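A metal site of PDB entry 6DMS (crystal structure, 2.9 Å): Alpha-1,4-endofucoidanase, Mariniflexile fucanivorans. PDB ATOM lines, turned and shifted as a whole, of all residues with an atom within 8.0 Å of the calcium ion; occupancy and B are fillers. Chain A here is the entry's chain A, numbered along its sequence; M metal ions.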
ATOM      1  N   ALA A 326       6.746  -2.390 -22.606  1.00  0.00           N
ATOM      2  CA  ALA A 326       6.285  -2.349 -21.213  1.00  0.00           C
ATOM      3  C   ALA A 326       6.815  -3.468 -20.310  1.00  0.00           C
ATOM      4  O   ALA A 326       7.113  -3.228 -19.140  1.00  0.00           O
ATOM      5  CB  ALA A 326       4.766  -2.312 -21.174  1.00  0.00           C
ATOM      6  N   PHE A 327       6.915  -4.688 -20.856  1.00  0.00           N
ATOM      7  CA  PHE A 327       7.212  -5.872 -20.037  1.00  0.00           C
ATOM      8  C   PHE A 327       8.409  -6.696 -20.528  1.00  0.00           C
ATOM      9  O   PHE A 327       8.273  -7.888 -20.850  1.00  0.00           O
ATOM     10  CB  PHE A 327       5.950  -6.745 -19.871  1.00  0.00           C
ATOM     11  CG  PHE A 327       4.737  -5.979 -19.457  1.00  0.00           C
ATOM     12  CD1 PHE A 327       4.616  -5.459 -18.162  1.00  0.00           C
ATOM     13  CD2 PHE A 327       3.698  -5.759 -20.361  1.00  0.00           C
ATOM     14  CE1 PHE A 327       3.489  -4.740 -17.785  1.00  0.00           C
ATOM     15  CE2 PHE A 327       2.568  -5.049 -19.999  1.00  0.00           C
ATOM     16  CZ  PHE A 327       2.460  -4.529 -18.706  1.00  0.00           C
ATOM     17  N   ARG A 328       9.582  -6.072 -20.576  1.00  0.00           N
ATOM     18  CA  ARG A 328      10.831  -6.785 -20.851  1.00  0.00           C
ATOM     19  C   ARG A 328      11.674  -6.976 -19.587  1.00  0.00           C
ATOM     20  O   ARG A 328      12.845  -7.376 -19.654  1.00  0.00           O
ATOM     21  CB  ARG A 328      11.610  -6.115 -21.991  1.00  0.00           C
ATOM     22  CG  ARG A 328      11.021  -6.388 -23.363  1.00  0.00           C
ATOM     23  CD  ARG A 328      11.983  -6.020 -24.471  1.00  0.00           C
ATOM     24  NE  ARG A 328      11.349  -6.145 -25.782  1.00  0.00           N
ATOM     25  CZ  ARG A 328      11.930  -5.889 -26.955  1.00  0.00           C
ATOM     26  NH1 ARG A 328      13.199  -5.501 -27.014  1.00  0.00           N
ATOM     27  NH2 ARG A 328      11.246  -6.042 -28.080  1.00  0.00           N
ATOM     28  N   ASP A 329      11.060  -6.684 -18.443  1.00  0.00           N
ATOM     29  CA  ASP A 329      11.690  -6.806 -17.130  1.00  0.00           C
ATOM     30  C   ASP A 329      11.325  -8.111 -16.404  1.00  0.00           C
ATOM     31  O   ASP A 329      12.153  -8.668 -15.676  1.00  0.00           O
ATOM     32  CB  ASP A 329      11.361  -5.593 -16.244  1.00  0.00           C
ATOM     33  CG  ASP A 329       9.849  -5.352 -16.105  1.00  0.00           C
ATOM     34  OD1 ASP A 329       9.145  -5.237 -17.129  1.00  0.00           O
ATOM     35  OD2 ASP A 329       9.378  -5.248 -14.949  1.00  0.00           O
ATOM     36  N   ASP A 330      10.101  -8.586 -16.625  1.00  0.00           N
ATOM     37  CA  ASP A 330       9.569  -9.776 -15.950  1.00  0.00           C
ATOM     38  C   ASP A 330      10.131 -11.105 -16.488  1.00  0.00           C
ATOM     39  O   ASP A 330      10.944 -11.116 -17.413  1.00  0.00           O
ATOM     40  CB  ASP A 330       8.024  -9.758 -15.970  1.00  0.00           C
ATOM     41  CG  ASP A 330       7.436  -9.948 -17.373  1.00  0.00           C
ATOM     42  OD1 ASP A 330       8.126  -9.716 -18.389  1.00  0.00           O
ATOM     43  OD2 ASP A 330       6.247 -10.323 -17.456  1.00  0.00           O
ATOM     44  N   THR A 331       9.686 -12.209 -15.891  1.00  0.00           N
ATOM     45  CA  THR A 331      10.159 -13.556 -16.221  1.00  0.00           C
ATOM     46  C   THR A 331       9.294 -14.277 -17.273  1.00  0.00           C
ATOM     47  O   THR A 331       9.321 -15.503 -17.386  1.00  0.00           O
ATOM     48  CB  THR A 331      10.296 -14.431 -14.947  1.00  0.00           C
ATOM     49  OG1 THR A 331       9.063 -14.414 -14.216  1.00  0.00           O
ATOM     50  CG2 THR A 331      11.429 -13.931 -14.054  1.00  0.00           C
ATOM     51  N   ARG A 332       8.539 -13.498 -18.050  1.00  0.00           N
ATOM     52  CA  ARG A 332       7.662 -14.031 -19.106  1.00  0.00           C
ATOM     53  C   ARG A 332       8.201 -13.727 -20.494  1.00  0.00           C
ATOM     54  O   ARG A 332       8.745 -12.646 -20.731  1.00  0.00           O
ATOM     55  CB  ARG A 332       6.241 -13.475 -18.967  1.00  0.00           C
ATOM     56  CG  ARG A 332       5.465 -14.034 -17.779  1.00  0.00           C
ATOM     57  CD  ARG A 332       4.078 -13.429 -17.692  1.00  0.00           C
ATOM     58  NE  ARG A 332       3.398 -13.829 -16.463  1.00  0.00           N
ATOM     59  CZ  ARG A 332       2.147 -13.514 -16.141  1.00  0.00           C
ATOM     60  NH1 ARG A 332       1.385 -12.783 -16.950  1.00  0.00           N
ATOM     61  NH2 ARG A 332       1.648 -13.941 -14.981  1.00  0.00           N
ATOM     62  N   THR A 333       8.038 -14.682 -21.406  1.00  0.00           N
ATOM     63  CA  THR A 333       8.580 -14.591 -22.767  1.00  0.00           C
ATOM     64  C   THR A 333       7.613 -13.990 -23.804  1.00  0.00           C
ATOM     65  O   THR A 333       8.036 -13.263 -24.707  1.00  0.00           O
ATOM     66  CB  THR A 333       9.151 -15.957 -23.256  1.00  0.00           C
ATOM     67  OG1 THR A 333       9.484 -15.878 -24.649  1.00  0.00           O
ATOM     68  CG2 THR A 333       8.158 -17.116 -23.023  1.00  0.00           C
ATOM     69  N   TRP A 334       6.330 -14.275 -23.641  1.00  0.00           N
ATOM     70  CA  TRP A 334       5.297 -13.949 -24.632  1.00  0.00           C
ATOM     71  C   TRP A 334       4.876 -12.466 -24.708  1.00  0.00           C
ATOM     72  O   TRP A 334       4.341 -12.034 -25.736  1.00  0.00           O
ATOM     73  CB  TRP A 334       4.056 -14.839 -24.433  1.00  0.00           C
ATOM     74  CG  TRP A 334       3.517 -14.850 -23.027  1.00  0.00           C
ATOM     75  CD1 TRP A 334       3.868 -15.717 -22.022  1.00  0.00           C
ATOM     76  CD2 TRP A 334       2.535 -13.965 -22.472  1.00  0.00           C
ATOM     77  NE1 TRP A 334       3.169 -15.420 -20.871  1.00  0.00           N
ATOM     78  CE2 TRP A 334       2.341 -14.356 -21.120  1.00  0.00           C
ATOM     79  CE3 TRP A 334       1.802 -12.881 -22.974  1.00  0.00           C
ATOM     80  CZ2 TRP A 334       1.436 -13.690 -20.266  1.00  0.00           C
ATOM     81  CZ3 TRP A 334       0.904 -12.221 -22.124  1.00  0.00           C
ATOM     82  CH2 TRP A 334       0.728 -12.632 -20.785  1.00  0.00           C
ATOM     83  N   ASN A 335       5.130 -11.713 -23.648  1.00  0.00           N
ATOM     84  CA  ASN A 335       4.748 -10.296 -23.560  1.00  0.00           C
ATOM     85  C   ASN A 335       5.856  -9.299 -23.964  1.00  0.00           C
ATOM     86  O   ASN A 335       5.731  -8.091 -23.729  1.00  0.00           O
ATOM     87  CB  ASN A 335       4.191  -9.955 -22.161  1.00  0.00           C
ATOM     88  CG  ASN A 335       5.158 -10.312 -21.027  1.00  0.00           C
ATOM     89  OD1 ASN A 335       6.375 -10.398 -21.208  1.00  0.00           O
ATOM     90  ND2 ASN A 335       4.596 -10.499 -19.837  1.00  0.00           N
ATOM     91  N   ASP A 336       6.915  -9.820 -24.595  1.00  0.00           N
ATOM     92  CA  ASP A 336       8.114  -9.041 -24.923  1.00  0.00           C
ATOM     93  C   ASP A 336       7.941  -7.989 -26.024  1.00  0.00           C
ATOM     94  O   ASP A 336       8.801  -7.112 -26.178  1.00  0.00           O
ATOM     95  CB  ASP A 336       9.274  -9.977 -25.268  1.00  0.00           C
ATOM     96  CG  ASP A 336       9.992 -10.515 -24.033  1.00  0.00           C
ATOM     97  OD1 ASP A 336       9.534 -10.266 -22.894  1.00  0.00           O
ATOM     98  OD2 ASP A 336      11.021 -11.191 -24.217  1.00  0.00           O
ATOM     99  N   ASN A 337       6.843  -8.062 -26.768  1.00  0.00           N
ATOM    100  CA  ASN A 337       6.564  -7.109 -27.847  1.00  0.00           C
ATOM    101  C   ASN A 337       5.477  -6.083 -27.510  1.00  0.00           C
ATOM    102  O   ASN A 337       5.194  -5.185 -28.313  1.00  0.00           O
ATOM    103  CB  ASN A 337       6.226  -7.850 -29.153  1.00  0.00           C
ATOM    104  CG  ASN A 337       7.415  -8.598 -29.731  1.00  0.00           C
ATOM    105  OD1 ASN A 337       7.343  -9.812 -29.942  1.00  0.00           O
ATOM    106  ND2 ASN A 337       8.505  -7.878 -29.987  1.00  0.00           N
HETATM  107 CA    CA M   1       8.975 -10.194 -20.604  1.00  0.00          CA
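The backbone carbonyl oxygen (O) of Asp 336 lies within hydrogen-bond range of the guanidinium group (NE) of Arg 328, 2.8 Å away.
Merely in contact with the calcium ion: Arg 328.
Within 4 Å of the calcium ion: Phe 327, Arg 328, Asp 330, Arg 332, Asn 335 and Asp 336.
The calcium ion is bound by OD1 of Asp 336 (2.4 Å), OD1 of Asp 330 (2.4 Å), O of Phe 327 (2.4 Å), O of Arg 332 (2.5 Å) and OD1 of Asn 335 (2.7 Å).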
